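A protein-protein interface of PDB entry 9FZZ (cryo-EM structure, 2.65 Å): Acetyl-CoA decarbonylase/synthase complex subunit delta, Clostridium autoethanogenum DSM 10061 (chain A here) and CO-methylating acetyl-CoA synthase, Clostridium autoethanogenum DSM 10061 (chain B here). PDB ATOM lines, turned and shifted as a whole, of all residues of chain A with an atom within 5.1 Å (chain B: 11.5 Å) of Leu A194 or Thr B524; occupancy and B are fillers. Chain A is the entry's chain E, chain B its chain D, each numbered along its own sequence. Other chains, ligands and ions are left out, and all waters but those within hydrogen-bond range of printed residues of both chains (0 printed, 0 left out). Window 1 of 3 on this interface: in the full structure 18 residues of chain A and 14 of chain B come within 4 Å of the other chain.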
ATOM      1  N   GLU A 159      23.206  27.831  -1.177  1.00  0.00           N
ATOM      2  CA  GLU A 159      23.872  26.562  -1.456  1.00  0.00           C
ATOM      3  C   GLU A 159      23.675  26.112  -2.897  1.00  0.00           C
ATOM      4  O   GLU A 159      24.513  25.384  -3.440  1.00  0.00           O
ATOM      5  CB  GLU A 159      23.359  25.487  -0.497  1.00  0.00           C
ATOM      6  CG  GLU A 159      24.066  24.145  -0.666  1.00  0.00           C
ATOM      7  CD  GLU A 159      23.385  23.041   0.112  1.00  0.00           C
ATOM      8  OE1 GLU A 159      22.346  23.322   0.735  1.00  0.00           O
ATOM      9  OE2 GLU A 159      23.886  21.897   0.096  1.00  0.00           O
ATOM     10  N   TYR A 162      26.331  28.449  -4.673  1.00  0.00           N
ATOM     11  CA  TYR A 162      27.439  28.971  -3.878  1.00  0.00           C
ATOM     12  C   TYR A 162      28.747  28.895  -4.653  1.00  0.00           C
ATOM     13  O   TYR A 162      29.591  29.791  -4.544  1.00  0.00           O
ATOM     14  CB  TYR A 162      27.536  28.234  -2.533  1.00  0.00           C
ATOM     15  CG  TYR A 162      28.237  26.899  -2.580  1.00  0.00           C
ATOM     16  CD1 TYR A 162      27.538  25.732  -2.883  1.00  0.00           C
ATOM     17  CD2 TYR A 162      29.602  26.798  -2.307  1.00  0.00           C
ATOM     18  CE1 TYR A 162      28.182  24.492  -2.926  1.00  0.00           C
ATOM     19  CE2 TYR A 162      30.260  25.571  -2.345  1.00  0.00           C
ATOM     20  CZ  TYR A 162      29.544  24.428  -2.655  1.00  0.00           C
ATOM     21  OH  TYR A 162      30.213  23.220  -2.689  1.00  0.00           O
ATOM     22  N   LYS A 189      26.046  26.635   9.248  1.00  0.00           N
ATOM     23  CA  LYS A 189      27.275  25.855   9.356  1.00  0.00           C
ATOM     24  C   LYS A 189      27.585  25.127   8.055  1.00  0.00           C
ATOM     25  O   LYS A 189      28.738  25.084   7.617  1.00  0.00           O
ATOM     26  CB  LYS A 189      27.169  24.846  10.501  1.00  0.00           C
ATOM     27  CG  LYS A 189      27.175  25.475  11.891  1.00  0.00           C
ATOM     28  CD  LYS A 189      26.840  24.436  12.976  1.00  0.00           C
ATOM     29  CE  LYS A 189      27.746  23.196  12.884  1.00  0.00           C
ATOM     30  NZ  LYS A 189      29.180  23.567  13.021  1.00  0.00           N
ATOM     31  N   GLN A 190      26.565  24.548   7.424  1.00  0.00           N
ATOM     32  CA  GLN A 190      26.786  23.792   6.194  1.00  0.00           C
ATOM     33  C   GLN A 190      27.276  24.692   5.071  1.00  0.00           C
ATOM     34  O   GLN A 190      28.205  24.328   4.341  1.00  0.00           O
ATOM     35  CB  GLN A 190      25.506  23.066   5.784  1.00  0.00           C
ATOM     36  CG  GLN A 190      25.693  22.175   4.552  1.00  0.00           C
ATOM     37  CD  GLN A 190      24.453  21.363   4.232  1.00  0.00           C
ATOM     38  OE1 GLN A 190      23.405  21.573   4.825  1.00  0.00           O
ATOM     39  NE2 GLN A 190      24.567  20.425   3.295  1.00  0.00           N
ATOM     40  N   ILE A 191      26.672  25.868   4.911  1.00  0.00           N
ATOM     41  CA  ILE A 191      27.104  26.761   3.840  1.00  0.00           C
ATOM     42  C   ILE A 191      28.501  27.299   4.130  1.00  0.00           C
ATOM     43  O   ILE A 191      29.324  27.431   3.219  1.00  0.00           O
ATOM     44  CB  ILE A 191      26.078  27.884   3.603  1.00  0.00           C
ATOM     45  CG1 ILE A 191      26.452  28.712   2.363  1.00  0.00           C
ATOM     46  CG2 ILE A 191      25.974  28.803   4.803  1.00  0.00           C
ATOM     47  CD1 ILE A 191      26.516  27.904   1.072  1.00  0.00           C
ATOM     48  N   ASN A 192      28.809  27.582   5.400  1.00  0.00           N
ATOM     49  CA  ASN A 192      30.157  28.037   5.739  1.00  0.00           C
ATOM     50  C   ASN A 192      31.193  26.950   5.466  1.00  0.00           C
ATOM     51  O   ASN A 192      32.286  27.236   4.964  1.00  0.00           O
ATOM     52  CB  ASN A 192      30.216  28.466   7.202  1.00  0.00           C
ATOM     53  CG  ASN A 192      29.426  29.732   7.478  1.00  0.00           C
ATOM     54  OD1 ASN A 192      28.690  30.197   6.621  1.00  0.00           O
ATOM     55  ND2 ASN A 192      29.578  30.294   8.672  1.00  0.00           N
ATOM     56  N   ILE A 193      30.870  25.700   5.794  1.00  0.00           N
ATOM     57  CA  ILE A 193      31.796  24.599   5.544  1.00  0.00           C
ATOM     58  C   ILE A 193      31.982  24.385   4.047  1.00  0.00           C
ATOM     59  O   ILE A 193      33.091  24.101   3.582  1.00  0.00           O
ATOM     60  CB  ILE A 193      31.312  23.324   6.253  1.00  0.00           C
ATOM     61  CG1 ILE A 193      31.420  23.508   7.775  1.00  0.00           C
ATOM     62  CG2 ILE A 193      32.126  22.114   5.801  1.00  0.00           C
ATOM     63  CD1 ILE A 193      30.828  22.352   8.574  1.00  0.00           C
ATOM     64  N   LEU A 194      30.906  24.506   3.270  1.00  0.00           N
ATOM     65  CA  LEU A 194      31.034  24.393   1.819  1.00  0.00           C
ATOM     66  C   LEU A 194      31.922  25.492   1.256  1.00  0.00           C
ATOM     67  O   LEU A 194      32.768  25.238   0.392  1.00  0.00           O
ATOM     68  CB  LEU A 194      29.655  24.432   1.158  1.00  0.00           C
ATOM     69  CG  LEU A 194      28.783  23.182   1.353  1.00  0.00           C
ATOM     70  CD1 LEU A 194      27.422  23.403   0.724  1.00  0.00           C
ATOM     71  CD2 LEU A 194      29.439  21.939   0.758  1.00  0.00           C
ATOM     72  N   MET A 195      31.752  26.722   1.739  1.00  0.00           N
ATOM     73  CA  MET A 195      32.596  27.819   1.273  1.00  0.00           C
ATOM     74  C   MET A 195      34.054  27.594   1.657  1.00  0.00           C
ATOM     75  O   MET A 195      34.963  27.880   0.871  1.00  0.00           O
ATOM     76  CB  MET A 195      32.097  29.148   1.845  1.00  0.00           C
ATOM     77  CG  MET A 195      30.682  29.525   1.400  1.00  0.00           C
ATOM     78  SD  MET A 195      30.606  30.009  -0.333  1.00  0.00           S
ATOM     79  CE  MET A 195      31.325  31.639  -0.280  1.00  0.00           C
ATOM     80  N   ASN A 196      34.300  27.093   2.871  1.00  0.00           N
ATOM     81  CA  ASN A 196      35.676  26.815   3.282  1.00  0.00           C
ATOM     82  C   ASN A 196      36.303  25.707   2.445  1.00  0.00           C
ATOM     83  O   ASN A 196      37.464  25.808   2.038  1.00  0.00           O
ATOM     84  CB  ASN A 196      35.716  26.447   4.763  1.00  0.00           C
ATOM     85  CG  ASN A 196      35.414  27.626   5.664  1.00  0.00           C
ATOM     86  OD1 ASN A 196      36.266  28.477   5.884  1.00  0.00           O
ATOM     87  ND2 ASN A 196      34.189  27.689   6.180  1.00  0.00           N
ATOM     88  N   GLN A 197      35.548  24.643   2.178  1.00  0.00           N
ATOM     89  CA  GLN A 197      36.072  23.557   1.356  1.00  0.00           C
ATOM     90  C   GLN A 197      36.293  23.997  -0.084  1.00  0.00           C
ATOM     91  O   GLN A 197      37.183  23.475  -0.762  1.00  0.00           O
ATOM     92  CB  GLN A 197      35.129  22.357   1.407  1.00  0.00           C
ATOM     93  CG  GLN A 197      35.090  21.680   2.777  1.00  0.00           C
ATOM     94  CD  GLN A 197      34.096  20.538   2.817  1.00  0.00           C
ATOM     95  OE1 GLN A 197      33.393  20.296   1.847  1.00  0.00           O
ATOM     96  NE2 GLN A 197      34.029  19.827   3.941  1.00  0.00           N
ATOM     97  N   LEU A 198      35.501  24.956  -0.561  1.00  0.00           N
ATOM     98  CA  LEU A 198      35.718  25.480  -1.902  1.00  0.00           C
ATOM     99  C   LEU A 198      37.068  26.173  -2.008  1.00  0.00           C
ATOM    100  O   LEU A 198      37.737  26.084  -3.043  1.00  0.00           O
ATOM    101  CB  LEU A 198      34.583  26.436  -2.277  1.00  0.00           C
ATOM    102  CG  LEU A 198      34.591  26.904  -3.738  1.00  0.00           C
ATOM    103  CD1 LEU A 198      34.539  25.715  -4.694  1.00  0.00           C
ATOM    104  CD2 LEU A 198      33.419  27.833  -3.995  1.00  0.00           C
ATOM    105  N   VAL B 128      35.265  26.111 -11.891  1.00  0.00           N
ATOM    106  CA  VAL B 128      34.891  25.792 -10.518  1.00  0.00           C
ATOM    107  C   VAL B 128      33.502  25.175 -10.470  1.00  0.00           C
ATOM    108  O   VAL B 128      33.263  24.204  -9.743  1.00  0.00           O
ATOM    109  CB  VAL B 128      34.990  27.046  -9.635  1.00  0.00           C
ATOM    110  CG1 VAL B 128      34.551  26.732  -8.204  1.00  0.00           C
ATOM    111  CG2 VAL B 128      36.419  27.591  -9.648  1.00  0.00           C
ATOM    112  N   PHE B 209      42.843  31.361  -7.839  1.00  0.00           N
ATOM    113  CA  PHE B 209      41.692  30.798  -7.145  1.00  0.00           C
ATOM    114  C   PHE B 209      42.078  30.029  -5.892  1.00  0.00           C
ATOM    115  O   PHE B 209      41.334  30.056  -4.906  1.00  0.00           O
ATOM    116  CB  PHE B 209      40.899  29.894  -8.094  1.00  0.00           C
ATOM    117  CG  PHE B 209      40.628  30.523  -9.436  1.00  0.00           C
ATOM    118  CD1 PHE B 209      39.751  31.599  -9.547  1.00  0.00           C
ATOM    119  CD2 PHE B 209      41.259  30.059 -10.580  1.00  0.00           C
ATOM    120  CE1 PHE B 209      39.496  32.210 -10.774  1.00  0.00           C
ATOM    121  CE2 PHE B 209      41.020  30.657 -11.826  1.00  0.00           C
ATOM    122  CZ  PHE B 209      40.137  31.743 -11.917  1.00  0.00           C
ATOM    123  N   ARG B 227      42.390  19.953  -8.260  1.00  0.00           N
ATOM    124  CA  ARG B 227      41.422  20.970  -8.651  1.00  0.00           C
ATOM    125  C   ARG B 227      41.322  21.215 -10.152  1.00  0.00           C
ATOM    126  O   ARG B 227      40.254  21.619 -10.617  1.00  0.00           O
ATOM    127  CB  ARG B 227      41.759  22.299  -7.968  1.00  0.00           C
ATOM    128  CG  ARG B 227      41.798  22.196  -6.448  1.00  0.00           C
ATOM    129  CD  ARG B 227      40.389  22.037  -5.876  1.00  0.00           C
ATOM    130  NE  ARG B 227      40.226  22.862  -4.686  1.00  0.00           N
ATOM    131  CZ  ARG B 227      39.104  22.973  -3.986  1.00  0.00           C
ATOM    132  NH1 ARG B 227      38.009  22.318  -4.321  1.00  0.00           N
ATOM    133  NH2 ARG B 227      39.084  23.769  -2.914  1.00  0.00           N
ATOM    134  N   SER B 436      27.824  10.722  -7.219  1.00  0.00           N
ATOM    135  CA  SER B 436      29.024  10.602  -6.403  1.00  0.00           C
ATOM    136  C   SER B 436      29.319   9.170  -5.977  1.00  0.00           C
ATOM    137  O   SER B 436      30.370   8.926  -5.379  1.00  0.00           O
ATOM    138  CB  SER B 436      28.899  11.466  -5.134  1.00  0.00           C
ATOM    139  OG  SER B 436      28.684  12.837  -5.454  1.00  0.00           O
ATOM    140  N   TYR B 483      26.492   6.546  14.243  1.00  0.00           N
ATOM    141  CA  TYR B 483      26.278   7.770  13.490  1.00  0.00           C
ATOM    142  C   TYR B 483      25.514   8.748  14.360  1.00  0.00           C
ATOM    143  O   TYR B 483      24.830   8.366  15.305  1.00  0.00           O
ATOM    144  CB  TYR B 483      25.524   7.498  12.175  1.00  0.00           C
ATOM    145  CG  TYR B 483      26.392   6.742  11.211  1.00  0.00           C
ATOM    146  CD1 TYR B 483      27.306   7.410  10.395  1.00  0.00           C
ATOM    147  CD2 TYR B 483      26.340   5.349  11.139  1.00  0.00           C
ATOM    148  CE1 TYR B 483      28.137   6.714   9.518  1.00  0.00           C
ATOM    149  CE2 TYR B 483      27.162   4.640  10.268  1.00  0.00           C
ATOM    150  CZ  TYR B 483      28.053   5.328   9.466  1.00  0.00           C
ATOM    151  OH  TYR B 483      28.857   4.604   8.610  1.00  0.00           O
ATOM    152  N   SER B 484      25.654  10.028  14.040  1.00  0.00           N
ATOM    153  CA  SER B 484      24.985  11.099  14.763  1.00  0.00           C
ATOM    154  C   SER B 484      24.192  11.917  13.758  1.00  0.00           C
ATOM    155  O   SER B 484      24.723  12.296  12.711  1.00  0.00           O
ATOM    156  CB  SER B 484      25.973  11.983  15.532  1.00  0.00           C
ATOM    157  OG  SER B 484      26.889  12.638  14.661  1.00  0.00           O
ATOM    158  N   CYS B 485      22.926  12.166  14.070  1.00  0.00           N
ATOM    159  CA  CYS B 485      22.046  12.972  13.246  1.00  0.00           C
ATOM    160  C   CYS B 485      21.529  14.121  14.098  1.00  0.00           C
ATOM    161  O   CYS B 485      21.098  13.904  15.235  1.00  0.00           O
ATOM    162  CB  CYS B 485      20.884  12.123  12.710  1.00  0.00           C
ATOM    163  SG  CYS B 485      19.860  12.948  11.474  1.00  0.00           S
ATOM    164  N   ASN B 486      21.577  15.342  13.555  1.00  0.00           N
ATOM    165  CA  ASN B 486      21.066  16.532  14.219  1.00  0.00           C
ATOM    166  C   ASN B 486      20.015  17.238  13.367  1.00  0.00           C
ATOM    167  O   ASN B 486      19.869  18.459  13.426  1.00  0.00           O
ATOM    168  CB  ASN B 486      22.196  17.498  14.582  1.00  0.00           C
ATOM    169  CG  ASN B 486      23.000  17.957  13.378  1.00  0.00           C
ATOM    170  OD1 ASN B 486      22.562  17.817  12.247  1.00  0.00           O
ATOM    171  ND2 ASN B 486      24.181  18.514  13.621  1.00  0.00           N
ATOM    172  N   LEU B 487      19.274  16.477  12.561  1.00  0.00           N
ATOM    173  CA  LEU B 487      18.276  17.071  11.684  1.00  0.00           C
ATOM    174  C   LEU B 487      17.123  17.690  12.454  1.00  0.00           C
ATOM    175  O   LEU B 487      16.468  18.598  11.936  1.00  0.00           O
ATOM    176  CB  LEU B 487      17.759  16.013  10.702  1.00  0.00           C
ATOM    177  CG  LEU B 487      16.874  16.518   9.555  1.00  0.00           C
ATOM    178  CD1 LEU B 487      17.624  17.514   8.679  1.00  0.00           C
ATOM    179  CD2 LEU B 487      16.392  15.347   8.719  1.00  0.00           C
ATOM    180  N   ALA B 515      21.866   6.052   7.784  1.00  0.00           N
ATOM    181  CA  ALA B 515      22.828   7.070   8.191  1.00  0.00           C
ATOM    182  C   ALA B 515      24.125   6.942   7.404  1.00  0.00           C
ATOM    183  O   ALA B 515      24.717   7.950   7.005  1.00  0.00           O
ATOM    184  CB  ALA B 515      23.098   6.967   9.692  1.00  0.00           C
ATOM    185  N   LYS B 516      24.588   5.714   7.181  1.00  0.00           N
ATOM    186  CA  LYS B 516      25.800   5.524   6.388  1.00  0.00           C
ATOM    187  C   LYS B 516      25.614   6.027   4.959  1.00  0.00           C
ATOM    188  O   LYS B 516      26.492   6.703   4.406  1.00  0.00           O
ATOM    189  CB  LYS B 516      26.197   4.049   6.395  1.00  0.00           C
ATOM    190  CG  LYS B 516      27.626   3.806   5.916  1.00  0.00           C
ATOM    191  CD  LYS B 516      28.146   2.450   6.412  1.00  0.00           C
ATOM    192  CE  LYS B 516      27.909   1.348   5.374  1.00  0.00           C
ATOM    193  NZ  LYS B 516      28.809   1.527   4.181  1.00  0.00           N
ATOM    194  N   ALA B 517      24.475   5.710   4.344  1.00  0.00           N
ATOM    195  CA  ALA B 517      24.207   6.177   2.986  1.00  0.00           C
ATOM    196  C   ALA B 517      24.095   7.695   2.933  1.00  0.00           C
ATOM    197  O   ALA B 517      24.598   8.326   1.998  1.00  0.00           O
ATOM    198  CB  ALA B 517      22.940   5.521   2.439  1.00  0.00           C
ATOM    199  N   THR B 518      23.436   8.300   3.923  1.00  0.00           N
ATOM    200  CA  THR B 518      23.317   9.755   3.955  1.00  0.00           C
ATOM    201  C   THR B 518      24.682  10.409   4.108  1.00  0.00           C
ATOM    202  O   THR B 518      24.980  11.399   3.436  1.00  0.00           O
ATOM    203  CB  THR B 518      22.399  10.196   5.099  1.00  0.00           C
ATOM    204  OG1 THR B 518      21.122   9.557   4.994  1.00  0.00           O
ATOM    205  CG2 THR B 518      22.190  11.698   5.059  1.00  0.00           C
ATOM    206  N   LEU B 519      25.534   9.852   4.964  1.00  0.00           N
ATOM    207  CA  LEU B 519      26.877  10.399   5.121  1.00  0.00           C
ATOM    208  C   LEU B 519      27.672  10.280   3.830  1.00  0.00           C
ATOM    209  O   LEU B 519      28.404  11.203   3.459  1.00  0.00           O
ATOM    210  CB  LEU B 519      27.601   9.690   6.268  1.00  0.00           C
ATOM    211  CG  LEU B 519      29.077  10.076   6.423  1.00  0.00           C
ATOM    212  CD1 LEU B 519      29.236  11.577   6.646  1.00  0.00           C
ATOM    213  CD2 LEU B 519      29.700   9.298   7.564  1.00  0.00           C
ATOM    214  N   GLU B 520      27.554   9.149   3.135  1.00  0.00           N
ATOM    215  CA  GLU B 520      28.300   8.973   1.892  1.00  0.00           C
ATOM    216  C   GLU B 520      27.811   9.924   0.805  1.00  0.00           C
ATOM    217  O   GLU B 520      28.615  10.561   0.118  1.00  0.00           O
ATOM    218  CB  GLU B 520      28.186   7.524   1.417  1.00  0.00           C
ATOM    219  CG  GLU B 520      28.919   7.267   0.096  1.00  0.00           C
ATOM    220  CD  GLU B 520      30.411   7.529   0.215  1.00  0.00           C
ATOM    221  OE1 GLU B 520      30.942   7.400   1.333  1.00  0.00           O
ATOM    222  OE2 GLU B 520      31.046   7.876  -0.802  1.00  0.00           O
ATOM    223  N   LEU B 521      26.495  10.027   0.630  1.00  0.00           N
ATOM    224  CA  LEU B 521      25.929  10.854  -0.432  1.00  0.00           C
ATOM    225  C   LEU B 521      25.977  12.340  -0.108  1.00  0.00           C
ATOM    226  O   LEU B 521      26.163  13.157  -1.015  1.00  0.00           O
ATOM    227  CB  LEU B 521      24.485  10.437  -0.716  1.00  0.00           C
ATOM    228  CG  LEU B 521      24.313   8.973  -1.140  1.00  0.00           C
ATOM    229  CD1 LEU B 521      22.841   8.665  -1.333  1.00  0.00           C
ATOM    230  CD2 LEU B 521      25.098   8.668  -2.414  1.00  0.00           C
ATOM    231  N   ASN B 522      25.817  12.709   1.160  1.00  0.00           N
ATOM    232  CA  ASN B 522      25.781  14.109   1.585  1.00  0.00           C
ATOM    233  C   ASN B 522      26.766  14.278   2.732  1.00  0.00           C
ATOM    234  O   ASN B 522      26.368  14.340   3.904  1.00  0.00           O
ATOM    235  CB  ASN B 522      24.361  14.497   1.996  1.00  0.00           C
ATOM    236  CG  ASN B 522      24.187  15.990   2.180  1.00  0.00           C
ATOM    237  OD1 ASN B 522      25.011  16.768   1.717  1.00  0.00           O
ATOM    238  ND2 ASN B 522      23.114  16.397   2.850  1.00  0.00           N
ATOM    239  N   PRO B 523      28.067  14.388   2.431  1.00  0.00           N
ATOM    240  CA  PRO B 523      29.060  14.451   3.526  1.00  0.00           C
ATOM    241  C   PRO B 523      28.874  15.619   4.477  1.00  0.00           C
ATOM    242  O   PRO B 523      29.164  15.474   5.671  1.00  0.00           O
ATOM    243  CB  PRO B 523      30.405  14.526   2.781  1.00  0.00           C
ATOM    244  CG  PRO B 523      30.064  15.029   1.397  1.00  0.00           C
ATOM    245  CD  PRO B 523      28.698  14.466   1.101  1.00  0.00           C
ATOM    246  N   THR B 524      28.398  16.770   4.004  1.00  0.00           N
ATOM    247  CA  THR B 524      28.140  17.916   4.866  1.00  0.00           C
ATOM    248  C   THR B 524      26.703  17.948   5.379  1.00  0.00           C
ATOM    249  O   THR B 524      26.199  19.022   5.725  1.00  0.00           O
ATOM    250  CB  THR B 524      28.461  19.225   4.139  1.00  0.00           C
ATOM    251  OG1 THR B 524      27.672  19.337   2.947  1.00  0.00           O
ATOM    252  CG2 THR B 524      29.928  19.283   3.775  1.00  0.00           C
ATOM    253  N   GLY B 525      26.040  16.798   5.442  1.00  0.00           N
ATOM    254  CA  GLY B 525      24.667  16.724   5.882  1.00  0.00           C
ATOM    255  C   GLY B 525      24.535  16.542   7.377  1.00  0.00           C
ATOM    256  O   GLY B 525      25.466  16.804   8.145  1.00  0.00           O
ATOM    257  N   PRO B 526      23.361  16.085   7.832  1.00  0.00           N
ATOM    258  CA  PRO B 526      23.150  15.918   9.279  1.00  0.00           C
ATOM    259  C   PRO B 526      23.725  14.639   9.858  1.00  0.00           C
ATOM    260  O   PRO B 526      23.956  14.588  11.072  1.00  0.00           O
ATOM    261  CB  PRO B 526      21.611  15.958   9.428  1.00  0.00           C
ATOM    262  CG  PRO B 526      21.044  16.098   7.998  1.00  0.00           C
ATOM    263  CD  PRO B 526      22.156  15.738   7.057  1.00  0.00           C
ATOM    264  N   CYS B 527      23.980  13.619   9.042  1.00  0.00           N
ATOM    265  CA  CYS B 527      24.483  12.342   9.530  1.00  0.00           C
ATOM    266  C   CYS B 527      26.003  12.328   9.421  1.00  0.00           C
ATOM    267  O   CYS B 527      26.555  12.480   8.328  1.00  0.00           O
ATOM    268  CB  CYS B 527      23.884  11.182   8.736  1.00  0.00           C
ATOM    269  SG  CYS B 527      22.107  10.981   8.947  1.00  0.00           S
ATOM    270  N   GLN B 528      26.673  12.138  10.558  1.00  0.00           N
ATOM    271  CA  GLN B 528      28.126  12.138  10.634  1.00  0.00           C
ATOM    272  C   GLN B 528      28.595  10.918  11.415  1.00  0.00           C
ATOM    273  O   GLN B 528      27.968  10.519  12.397  1.00  0.00           O
ATOM    274  CB  GLN B 528      28.645  13.422  11.304  1.00  0.00           C
ATOM    275  CG  GLN B 528      28.257  14.709  10.550  1.00  0.00           C
ATOM    276  CD  GLN B 528      28.914  14.813   9.175  1.00  0.00           C
ATOM    277  OE1 GLN B 528      30.038  14.367   8.985  1.00  0.00           O
ATOM    278  NE2 GLN B 528      28.205  15.397   8.208  1.00  0.00           N
ATOM    279  N   ALA B 529      29.714  10.348  10.988  1.00  0.00           N
ATOM    280  CA  ALA B 529      30.234   9.141  11.616  1.00  0.00           C
ATOM    281  C   ALA B 529      30.775   9.438  13.008  1.00  0.00           C
ATOM    282  O   ALA B 529      31.398  10.480  13.235  1.00  0.00           O
ATOM    283  CB  ALA B 529      31.331   8.518  10.753  1.00  0.00           C
ATOM    284  N   ILE B 553      28.168  18.501  19.024  1.00  0.00           N
ATOM    285  CA  ILE B 553      27.031  18.719  18.133  1.00  0.00           C
ATOM    286  C   ILE B 553      25.945  19.535  18.818  1.00  0.00           C
ATOM    287  O   ILE B 553      25.357  20.437  18.211  1.00  0.00           O
ATOM    288  CB  ILE B 553      26.497  17.374  17.618  1.00  0.00           C
ATOM    289  CG1 ILE B 553      27.567  16.707  16.740  1.00  0.00           C
ATOM    290  CG2 ILE B 553      25.205  17.582  16.840  1.00  0.00           C
ATOM    291  CD1 ILE B 553      27.111  15.419  16.081  1.00  0.00           C
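No residue of chain B comes within 4 Å of Glu A159. Of the printed residues of chain B, Gln A190 touches Thr B524. No residue of chain B comes within 4 Å of Ile A191. No residue of chain B comes within 4 Å of Ile A193. Leu A194 touches just one residue of chain B: Thr B524. No residue of chain B comes within 4 Å of Met A195. No residue of chain B comes within 4 Å of Asn A196. Of chain B, only Val B128 and Arg B227 come within 4 Å of Leu A198. Printed residues of chain A within 4 Å of Val B128: Leu A198 (3.7 Å). Printed residues of chain A within 4 Å of Arg B227: Gln A197 and Leu A198. Ala B517 touches none of the printed residues of chain A. Glu B520 touches none of the printed residues of chain A. Of chain A, only Gln A190 and Leu A194 come within 4 Å of Thr B524. The nearest residue of chain B that does not touch Leu A194 is Asn B522 (6.9 Å). The nearest printed residue of chain A that does not touch Thr B524 is Gln A197 (4.1 Å).
CD2 of Leu A194 touches OG1 of Thr B524, at 3.8 Å. Leu A198 touches Val B128 (CD1 to CG1, 3.7 Å).
Hydrophobic or aromatic side chains of chain B within 4 Å of the printed part of chain A: Val B128. Of the 12 printed residues of chain A, 4 touch a printed residue of chain B. Hydrophobic or aromatic side chains of chain A within 4 Å of the printed part of chain B: Leu A194 and Leu A198. Among the printed residues, 5 pairs touch across the chains. Among the printed residues, no Asp or Glu carboxylate lies within 4 Å of a Lys or Arg side-chain nitrogen of the other chain.
The backbone carbonyl oxygen of Gln A197 lies within hydrogen-bond range of the guanidinium group of Arg B227 (2.9 Å). The backbone carbonyl oxygen (O) of Thr B524 lies within hydrogen-bond range of the side-chain amide nitrogen (NE2) of Gln A190. NH2 of Arg B227 lies within hydrogen-bond range of O of Leu A198.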
